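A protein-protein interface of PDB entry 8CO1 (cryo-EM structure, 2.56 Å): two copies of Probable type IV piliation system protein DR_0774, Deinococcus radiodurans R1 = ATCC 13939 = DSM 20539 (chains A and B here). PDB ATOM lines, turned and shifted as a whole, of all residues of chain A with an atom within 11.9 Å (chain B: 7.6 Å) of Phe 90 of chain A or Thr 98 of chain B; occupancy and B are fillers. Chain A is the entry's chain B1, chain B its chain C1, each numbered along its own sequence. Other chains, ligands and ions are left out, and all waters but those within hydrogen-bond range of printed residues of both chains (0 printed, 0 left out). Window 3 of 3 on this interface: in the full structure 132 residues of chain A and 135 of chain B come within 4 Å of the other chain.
O of Lys 52 of chain B lies close to OD1 of Asn 85 of chain A (2.9 Å).
O of Lys 52 of chain B is in hydrogen-bond range of N of Gly 86 of chain A, 2.7 Å away.
Among the printed residues, merely in contact across the chains: Ile 84 of chain A with Val 54 of chain B, Ile 84 of chain A with Tyr 101 of chain B, Asn 85 of chain A with Val 54 of chain B, Val 89 of chain A with Val 54 of chain B, Phe 90 of chain A with Val 54 of chain B and Phe 90 of chain A with Thr 98 of chain B.
The backbone NH of Ser 100 of chain B lies within hydrogen-bond range of the side-chain hydroxyl of Thr 98 of chain B (3.2 Å).
Phe 90 of chain A touches just these residues of chain B: Val 54 and Thr 98.
Of chain A, only Phe 90 (3.8 Å) comes within 4 Å of Thr 98 of chain B.
No residue of chain B comes within 4 Å of Gly 91 of chain A.
Val 54 of chain B touches four residues of chain A.
No residue of chain A comes within 4 Å of Gly 55 of chain B.
No residue of chain A comes within 4 Å of Gly 91 of chain B.
No residue of chain A comes within 4 Å of Thr 99 of chain B.
Of the printed residues of chain A, Tyr 101 of chain B touches Ile 84 (3.7 Å).
Of the printed residues of chain B, Gly 86 of chain A touches Lys 52.
Of the printed residues of chain B, Asn 85 of chain A touches Lys 52 and Val 54.
Of the printed residues of chain B, Ile 84 of chain A touches Val 54 (3.9 Å) and Tyr 101 (3.7 Å).
Pro 104 of chain A touches none of the printed residues of chain B.
The nearest printed residue of chain B that does not touch Val 89 of chain A is Tyr 101 of chain B (4.8 Å).
Phe 90 of chain A touches Thr 98 of chain B, but with the chains exchanged Thr 98 of chain A does not touch Phe 90 of chain B (24.3 Å).
9 positions are printed for both chains.
Of the 8 pairs that touch across the chains among the printed residues, none has its exchanged pair printed and touching as well.
Hydrophobic or aromatic side chains of chain A within 4 Å of the printed part of chain B: Ile 84, Val 89 and Phe 90.
Along chain A the printed residues that touch a printed residue of chain B span positions 84 to 90.
Of the 13 printed residues of chain B, 4 touch a printed residue of chain A.
Hydrophobic or aromatic side chains of chain B that line the printed part of chain A: Val 54 and Tyr 101.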
ATOM      1  N   PRO A  56       5.210  -1.486 -12.043  1.00  0.00           N
ATOM      2  CA  PRO A  56       6.115  -1.855 -10.951  1.00  0.00           C
ATOM      3  C   PRO A  56       6.329  -3.346 -10.826  1.00  0.00           C
ATOM      4  O   PRO A  56       7.300  -3.759 -10.180  1.00  0.00           O
ATOM      5  CB  PRO A  56       5.408  -1.294  -9.717  1.00  0.00           C
ATOM      6  CG  PRO A  56       3.969  -1.394 -10.063  1.00  0.00           C
ATOM      7  CD  PRO A  56       3.849  -1.215 -11.557  1.00  0.00           C
ATOM      8  N   LEU A  83      -3.141  -4.488  -9.127  1.00  0.00           N
ATOM      9  CA  LEU A  83      -1.981  -4.370  -8.257  1.00  0.00           C
ATOM     10  C   LEU A  83      -2.131  -3.152  -7.363  1.00  0.00           C
ATOM     11  O   LEU A  83      -2.513  -2.077  -7.828  1.00  0.00           O
ATOM     12  CB  LEU A  83      -0.695  -4.262  -9.066  1.00  0.00           C
ATOM     13  CG  LEU A  83      -0.551  -5.236 -10.233  1.00  0.00           C
ATOM     14  CD1 LEU A  83       0.444  -4.707 -11.235  1.00  0.00           C
ATOM     15  CD2 LEU A  83      -0.133  -6.596  -9.734  1.00  0.00           C
ATOM     16  N   ILE A  84      -1.817  -3.324  -6.083  1.00  0.00           N
ATOM     17  CA  ILE A  84      -1.946  -2.276  -5.079  1.00  0.00           C
ATOM     18  C   ILE A  84      -0.603  -2.096  -4.389  1.00  0.00           C
ATOM     19  O   ILE A  84       0.096  -3.073  -4.103  1.00  0.00           O
ATOM     20  CB  ILE A  84      -3.061  -2.604  -4.063  1.00  0.00           C
ATOM     21  CG1 ILE A  84      -3.208  -1.492  -3.033  1.00  0.00           C
ATOM     22  CG2 ILE A  84      -2.814  -3.926  -3.390  1.00  0.00           C
ATOM     23  CD1 ILE A  84      -3.851  -0.273  -3.569  1.00  0.00           C
ATOM     24  N   ASN A  85      -0.232  -0.847  -4.141  1.00  0.00           N
ATOM     25  CA  ASN A  85       1.093  -0.524  -3.638  1.00  0.00           C
ATOM     26  C   ASN A  85       1.040   0.853  -3.000  1.00  0.00           C
ATOM     27  O   ASN A  85       0.068   1.593  -3.156  1.00  0.00           O
ATOM     28  CB  ASN A  85       2.131  -0.560  -4.759  1.00  0.00           C
ATOM     29  CG  ASN A  85       3.532  -0.731  -4.250  1.00  0.00           C
ATOM     30  OD1 ASN A  85       3.794  -0.561  -3.064  1.00  0.00           O
ATOM     31  ND2 ASN A  85       4.449  -1.057  -5.147  1.00  0.00           N
ATOM     32  N   GLY A  86       2.099   1.189  -2.270  1.00  0.00           N
ATOM     33  CA  GLY A  86       2.187   2.523  -1.707  1.00  0.00           C
ATOM     34  C   GLY A  86       2.325   3.589  -2.774  1.00  0.00           C
ATOM     35  O   GLY A  86       1.704   4.650  -2.689  1.00  0.00           O
ATOM     36  N   GLU A  87       3.138   3.324  -3.793  1.00  0.00           N
ATOM     37  CA  GLU A  87       3.360   4.286  -4.861  1.00  0.00           C
ATOM     38  C   GLU A  87       2.239   4.289  -5.889  1.00  0.00           C
ATOM     39  O   GLU A  87       2.002   5.320  -6.527  1.00  0.00           O
ATOM     40  CB  GLU A  87       4.700   3.995  -5.541  1.00  0.00           C
ATOM     41  CG  GLU A  87       4.965   4.791  -6.801  1.00  0.00           C
ATOM     42  CD  GLU A  87       5.920   4.087  -7.739  1.00  0.00           C
ATOM     43  OE1 GLU A  87       5.813   2.850  -7.876  1.00  0.00           O
ATOM     44  OE2 GLU A  87       6.774   4.769  -8.343  1.00  0.00           O
ATOM     45  N   ILE A  88       1.530   3.172  -6.048  1.00  0.00           N
ATOM     46  CA  ILE A  88       0.484   3.089  -7.061  1.00  0.00           C
ATOM     47  C   ILE A  88      -0.632   4.083  -6.772  1.00  0.00           C
ATOM     48  O   ILE A  88      -1.145   4.742  -7.681  1.00  0.00           O
ATOM     49  CB  ILE A  88      -0.049   1.649  -7.152  1.00  0.00           C
ATOM     50  CG1 ILE A  88       0.967   0.753  -7.854  1.00  0.00           C
ATOM     51  CG2 ILE A  88      -1.375   1.618  -7.869  1.00  0.00           C
ATOM     52  CD1 ILE A  88       0.564  -0.697  -7.890  1.00  0.00           C
ATOM     53  N   VAL A  89      -1.025   4.213  -5.509  1.00  0.00           N
ATOM     54  CA  VAL A  89      -2.155   5.074  -5.184  1.00  0.00           C
ATOM     55  C   VAL A  89      -1.728   6.481  -4.786  1.00  0.00           C
ATOM     56  O   VAL A  89      -2.493   7.431  -4.972  1.00  0.00           O
ATOM     57  CB  VAL A  89      -3.010   4.435  -4.080  1.00  0.00           C
ATOM     58  CG1 VAL A  89      -3.400   3.045  -4.477  1.00  0.00           C
ATOM     59  CG2 VAL A  89      -2.260   4.408  -2.778  1.00  0.00           C
ATOM     60  N   PHE A  90      -0.525   6.648  -4.245  1.00  0.00           N
ATOM     61  CA  PHE A  90      -0.101   7.924  -3.690  1.00  0.00           C
ATOM     62  C   PHE A  90       0.870   8.669  -4.591  1.00  0.00           C
ATOM     63  O   PHE A  90       1.471   9.654  -4.153  1.00  0.00           O
ATOM     64  CB  PHE A  90       0.524   7.712  -2.312  1.00  0.00           C
ATOM     65  CG  PHE A  90      -0.451   7.248  -1.275  1.00  0.00           C
ATOM     66  CD1 PHE A  90      -1.758   7.697  -1.287  1.00  0.00           C
ATOM     67  CD2 PHE A  90      -0.062   6.363  -0.287  1.00  0.00           C
ATOM     68  CE1 PHE A  90      -2.656   7.272  -0.336  1.00  0.00           C
ATOM     69  CE2 PHE A  90      -0.957   5.936   0.666  1.00  0.00           C
ATOM     70  CZ  PHE A  90      -2.255   6.391   0.642  1.00  0.00           C
ATOM     71  N   GLY A  91       1.036   8.234  -5.834  1.00  0.00           N
ATOM     72  CA  GLY A  91       2.018   8.887  -6.668  1.00  0.00           C
ATOM     73  C   GLY A  91       3.433   8.622  -6.172  1.00  0.00           C
ATOM     74  O   GLY A  91       3.717   7.638  -5.485  1.00  0.00           O
ATOM     75  N   ASN A  92       4.330   9.532  -6.531  1.00  0.00           N
ATOM     76  CA  ASN A  92       5.731   9.407  -6.150  1.00  0.00           C
ATOM     77  C   ASN A  92       6.374  10.776  -5.963  1.00  0.00           C
ATOM     78  O   ASN A  92       6.063  11.494  -5.013  1.00  0.00           O
ATOM     79  CB  ASN A  92       6.496   8.601  -7.201  1.00  0.00           C
ATOM     80  CG  ASN A  92       7.785   8.014  -6.660  1.00  0.00           C
ATOM     81  OD1 ASN A  92       8.009   7.984  -5.449  1.00  0.00           O
ATOM     82  ND2 ASN A  92       8.641   7.541  -7.558  1.00  0.00           N
ATOM     83  N   THR A  98       5.012  10.157 -12.444  1.00  0.00           N
ATOM     84  CA  THR A  98       4.032   9.775 -13.453  1.00  0.00           C
ATOM     85  C   THR A  98       2.631   9.727 -12.859  1.00  0.00           C
ATOM     86  O   THR A  98       2.385  10.267 -11.781  1.00  0.00           O
ATOM     87  CB  THR A  98       4.362   8.405 -14.076  1.00  0.00           C
ATOM     88  OG1 THR A  98       4.078   7.367 -13.130  1.00  0.00           O
ATOM     89  CG2 THR A  98       5.830   8.339 -14.467  1.00  0.00           C
ATOM     90  N   THR A  99       1.713   9.073 -13.570  1.00  0.00           N
ATOM     91  CA  THR A  99       0.328   8.959 -13.136  1.00  0.00           C
ATOM     92  C   THR A  99      -0.007   7.535 -12.695  1.00  0.00           C
ATOM     93  O   THR A  99      -1.183   7.184 -12.559  1.00  0.00           O
ATOM     94  CB  THR A  99      -0.605   9.438 -14.253  1.00  0.00           C
ATOM     95  OG1 THR A  99      -0.090  10.658 -14.797  1.00  0.00           O
ATOM     96  CG2 THR A  99      -1.999   9.746 -13.709  1.00  0.00           C
ATOM     97  N   SER A 100       1.013   6.708 -12.460  1.00  0.00           N
ATOM     98  CA  SER A 100       0.852   5.409 -11.809  1.00  0.00           C
ATOM     99  C   SER A 100      -0.090   4.496 -12.602  1.00  0.00           C
ATOM    100  O   SER A 100      -1.203   4.177 -12.184  1.00  0.00           O
ATOM    101  CB  SER A 100       0.363   5.585 -10.369  1.00  0.00           C
ATOM    102  OG  SER A 100       1.275   6.367  -9.618  1.00  0.00           O
ATOM    103  N   TYR A 101       0.398   4.079 -13.769  1.00  0.00           N
ATOM    104  CA  TYR A 101      -0.339   3.160 -14.626  1.00  0.00           C
ATOM    105  C   TYR A 101      -0.410   1.787 -13.967  1.00  0.00           C
ATOM    106  O   TYR A 101       0.263   0.850 -14.398  1.00  0.00           O
ATOM    107  CB  TYR A 101       0.347   3.082 -15.997  1.00  0.00           C
ATOM    108  CG  TYR A 101      -0.249   2.115 -17.001  1.00  0.00           C
ATOM    109  CD1 TYR A 101      -1.331   2.477 -17.781  1.00  0.00           C
ATOM    110  CD2 TYR A 101       0.304   0.861 -17.204  1.00  0.00           C
ATOM    111  CE1 TYR A 101      -1.863   1.606 -18.700  1.00  0.00           C
ATOM    112  CE2 TYR A 101      -0.227  -0.013 -18.111  1.00  0.00           C
ATOM    113  CZ  TYR A 101      -1.306   0.363 -18.858  1.00  0.00           C
ATOM    114  OH  TYR A 101      -1.828  -0.512 -19.772  1.00  0.00           O
ATOM    115  N   ALA A 102      -1.152   1.667 -12.867  1.00  0.00           N
ATOM    116  CA  ALA A 102      -1.361   0.348 -12.283  1.00  0.00           C
ATOM    117  C   ALA A 102      -2.817   0.077 -11.924  1.00  0.00           C
ATOM    118  O   ALA A 102      -3.301  -1.041 -12.123  1.00  0.00           O
ATOM    119  CB  ALA A 102      -0.478   0.181 -11.057  1.00  0.00           C
ATOM    120  N   THR A 103      -3.515   1.087 -11.396  1.00  0.00           N
ATOM    121  CA  THR A 103      -4.963   1.057 -11.204  1.00  0.00           C
ATOM    122  C   THR A 103      -5.436  -0.174 -10.435  1.00  0.00           C
ATOM    123  O   THR A 103      -5.824  -1.171 -11.053  1.00  0.00           O
ATOM    124  CB  THR A 103      -5.677   1.142 -12.551  1.00  0.00           C
ATOM    125  OG1 THR A 103      -5.224   2.309 -13.243  1.00  0.00           O
ATOM    126  CG2 THR A 103      -7.173   1.282 -12.340  1.00  0.00           C
ATOM    127  N   PRO A 104      -5.364  -0.167  -9.096  1.00  0.00           N
ATOM    128  CA  PRO A 104      -5.774  -1.340  -8.301  1.00  0.00           C
ATOM    129  C   PRO A 104      -7.087  -1.983  -8.721  1.00  0.00           C
ATOM    130  O   PRO A 104      -7.359  -3.130  -8.361  1.00  0.00           O
ATOM    131  CB  PRO A 104      -5.892  -0.778  -6.880  1.00  0.00           C
ATOM    132  CG  PRO A 104      -5.115   0.464  -6.878  1.00  0.00           C
ATOM    133  CD  PRO A 104      -5.097   1.011  -8.259  1.00  0.00           C
ATOM    134  N   LYS B  52       5.979  -0.372  -0.929  1.00  0.00           N
ATOM    135  CA  LYS B  52       5.640  -0.256   0.481  1.00  0.00           C
ATOM    136  C   LYS B  52       4.140  -0.442   0.643  1.00  0.00           C
ATOM    137  O   LYS B  52       3.362  -0.125  -0.257  1.00  0.00           O
ATOM    138  CB  LYS B  52       6.052   1.098   1.056  1.00  0.00           C
ATOM    139  CG  LYS B  52       7.417   1.574   0.609  1.00  0.00           C
ATOM    140  CD  LYS B  52       8.514   1.006   1.492  1.00  0.00           C
ATOM    141  CE  LYS B  52       9.812   0.840   0.719  1.00  0.00           C
ATOM    142  NZ  LYS B  52      10.089   2.011  -0.157  1.00  0.00           N
ATOM    143  N   TYR B  53       3.742  -0.959   1.798  1.00  0.00           N
ATOM    144  CA  TYR B  53       2.331  -1.192   2.061  1.00  0.00           C
ATOM    145  C   TYR B  53       1.585   0.129   2.182  1.00  0.00           C
ATOM    146  O   TYR B  53       2.135   1.142   2.618  1.00  0.00           O
ATOM    147  CB  TYR B  53       2.158  -2.011   3.333  1.00  0.00           C
ATOM    148  CG  TYR B  53       2.622  -3.436   3.193  1.00  0.00           C
ATOM    149  CD1 TYR B  53       1.909  -4.343   2.428  1.00  0.00           C
ATOM    150  CD2 TYR B  53       3.778  -3.872   3.817  1.00  0.00           C
ATOM    151  CE1 TYR B  53       2.327  -5.645   2.298  1.00  0.00           C
ATOM    152  CE2 TYR B  53       4.205  -5.170   3.691  1.00  0.00           C
ATOM    153  CZ  TYR B  53       3.476  -6.052   2.930  1.00  0.00           C
ATOM    154  OH  TYR B  53       3.901  -7.350   2.799  1.00  0.00           O
ATOM    155  N   VAL B  54       0.315   0.111   1.794  1.00  0.00           N
ATOM    156  CA  VAL B  54      -0.460   1.346   1.725  1.00  0.00           C
ATOM    157  C   VAL B  54      -1.305   1.562   2.974  1.00  0.00           C
ATOM    158  O   VAL B  54      -1.353   2.671   3.509  1.00  0.00           O
ATOM    159  CB  VAL B  54      -1.318   1.355   0.445  1.00  0.00           C
ATOM    160  CG1 VAL B  54      -2.263   0.184   0.414  1.00  0.00           C
ATOM    161  CG2 VAL B  54      -2.104   2.634   0.368  1.00  0.00           C
ATOM    162  N   GLY B  55      -1.972   0.529   3.472  1.00  0.00           N
ATOM    163  CA  GLY B  55      -2.936   0.702   4.529  1.00  0.00           C
ATOM    164  C   GLY B  55      -2.314   0.711   5.904  1.00  0.00           C
ATOM    165  O   GLY B  55      -1.103   0.541   6.067  1.00  0.00           O
ATOM    166  N   GLU B  87      -6.965   7.871  12.674  1.00  0.00           N
ATOM    167  CA  GLU B  87      -6.311   8.490  11.529  1.00  0.00           C
ATOM    168  C   GLU B  87      -7.067   8.263  10.229  1.00  0.00           C
ATOM    169  O   GLU B  87      -6.952   9.079   9.310  1.00  0.00           O
ATOM    170  CB  GLU B  87      -4.884   7.954  11.406  1.00  0.00           C
ATOM    171  CG  GLU B  87      -4.110   8.466  10.212  1.00  0.00           C
ATOM    172  CD  GLU B  87      -3.117   7.450   9.691  1.00  0.00           C
ATOM    173  OE1 GLU B  87      -2.133   7.856   9.038  1.00  0.00           O
ATOM    174  OE2 GLU B  87      -3.319   6.243   9.940  1.00  0.00           O
ATOM    175  N   PHE B  90      -9.913  11.082  10.259  1.00  0.00           N
ATOM    176  CA  PHE B  90      -9.521  12.445  10.580  1.00  0.00           C
ATOM    177  C   PHE B  90      -8.245  12.878   9.875  1.00  0.00           C
ATOM    178  O   PHE B  90      -7.682  13.919  10.222  1.00  0.00           O
ATOM    179  CB  PHE B  90      -9.359  12.598  12.092  1.00  0.00           C
ATOM    180  CG  PHE B  90     -10.644  12.465  12.849  1.00  0.00           C
ATOM    181  CD1 PHE B  90     -11.826  12.940  12.314  1.00  0.00           C
ATOM    182  CD2 PHE B  90     -10.672  11.868  14.094  1.00  0.00           C
ATOM    183  CE1 PHE B  90     -13.010  12.819  13.004  1.00  0.00           C
ATOM    184  CE2 PHE B  90     -11.852  11.746  14.789  1.00  0.00           C
ATOM    185  CZ  PHE B  90     -13.022  12.222  14.243  1.00  0.00           C
ATOM    186  N   GLY B  91      -7.778  12.115   8.896  1.00  0.00           N
ATOM    187  CA  GLY B  91      -6.525  12.475   8.274  1.00  0.00           C
ATOM    188  C   GLY B  91      -5.357  12.306   9.236  1.00  0.00           C
ATOM    189  O   GLY B  91      -5.398  11.529  10.191  1.00  0.00           O
ATOM    190  N   ASN B  92      -4.301  13.065   8.968  1.00  0.00           N
ATOM    191  CA  ASN B  92      -3.095  12.997   9.782  1.00  0.00           C
ATOM    192  C   ASN B  92      -2.378  14.342   9.815  1.00  0.00           C
ATOM    193  O   ASN B  92      -2.872  15.305  10.402  1.00  0.00           O
ATOM    194  CB  ASN B  92      -2.158  11.912   9.251  1.00  0.00           C
ATOM    195  CG  ASN B  92      -1.153  11.451  10.287  1.00  0.00           C
ATOM    196  OD1 ASN B  92      -1.285  11.748  11.475  1.00  0.00           O
ATOM    197  ND2 ASN B  92      -0.140  10.716   9.842  1.00  0.00           N
ATOM    198  N   THR B  98      -1.845  12.027   3.602  1.00  0.00           N
ATOM    199  CA  THR B  98      -2.521  11.420   2.461  1.00  0.00           C
ATOM    200  C   THR B  98      -4.030  11.581   2.575  1.00  0.00           C
ATOM    201  O   THR B  98      -4.520  12.403   3.350  1.00  0.00           O
ATOM    202  CB  THR B  98      -2.182   9.924   2.330  1.00  0.00           C
ATOM    203  OG1 THR B  98      -2.852   9.187   3.361  1.00  0.00           O
ATOM    204  CG2 THR B  98      -0.682   9.705   2.449  1.00  0.00           C
ATOM    205  N   THR B  99      -4.767  10.787   1.800  1.00  0.00           N
ATOM    206  CA  THR B  99      -6.221  10.843   1.787  1.00  0.00           C
ATOM    207  C   THR B  99      -6.836   9.608   2.445  1.00  0.00           C
ATOM    208  O   THR B  99      -8.034   9.349   2.290  1.00  0.00           O
ATOM    209  CB  THR B  99      -6.721  11.025   0.351  1.00  0.00           C
ATOM    210  OG1 THR B  99      -5.926  12.025  -0.294  1.00  0.00           O
ATOM    211  CG2 THR B  99      -8.166  11.521   0.332  1.00  0.00           C
ATOM    212  N   SER B 100      -6.034   8.844   3.188  1.00  0.00           N
ATOM    213  CA  SER B 100      -6.530   7.780   4.061  1.00  0.00           C
ATOM    214  C   SER B 100      -7.299   6.717   3.270  1.00  0.00           C
ATOM    215  O   SER B 100      -8.514   6.562   3.386  1.00  0.00           O
ATOM    216  CB  SER B 100      -7.394   8.364   5.183  1.00  0.00           C
ATOM    217  OG  SER B 100      -6.656   9.290   5.959  1.00  0.00           O
ATOM    218  N   TYR B 101      -6.545   5.980   2.458  1.00  0.00           N
ATOM    219  CA  TYR B 101      -7.105   4.891   1.668  1.00  0.00           C
ATOM    220  C   TYR B 101      -7.526   3.748   2.587  1.00  0.00           C
ATOM    221  O   TYR B 101      -6.873   2.705   2.628  1.00  0.00           O
ATOM    222  CB  TYR B 101      -6.065   4.423   0.641  1.00  0.00           C
ATOM    223  CG  TYR B 101      -6.450   3.237  -0.220  1.00  0.00           C
ATOM    224  CD1 TYR B 101      -7.228   3.401  -1.349  1.00  0.00           C
ATOM    225  CD2 TYR B 101      -5.989   1.963   0.069  1.00  0.00           C
ATOM    226  CE1 TYR B 101      -7.567   2.328  -2.137  1.00  0.00           C
ATOM    227  CE2 TYR B 101      -6.329   0.890  -0.709  1.00  0.00           C
ATOM    228  CZ  TYR B 101      -7.114   1.076  -1.810  1.00  0.00           C
ATOM    229  OH  TYR B 101      -7.446   0.001  -2.589  1.00  0.00           O
ATOM    230  N   ALA B 102      -8.566   3.955   3.395  1.00  0.00           N
ATOM    231  CA  ALA B 102      -9.099   2.846   4.177  1.00  0.00           C
ATOM    232  C   ALA B 102     -10.618   2.743   4.109  1.00  0.00           C
ATOM    233  O   ALA B 102     -11.155   1.634   4.032  1.00  0.00           O
ATOM    234  CB  ALA B 102      -8.646   2.967   5.622  1.00  0.00           C
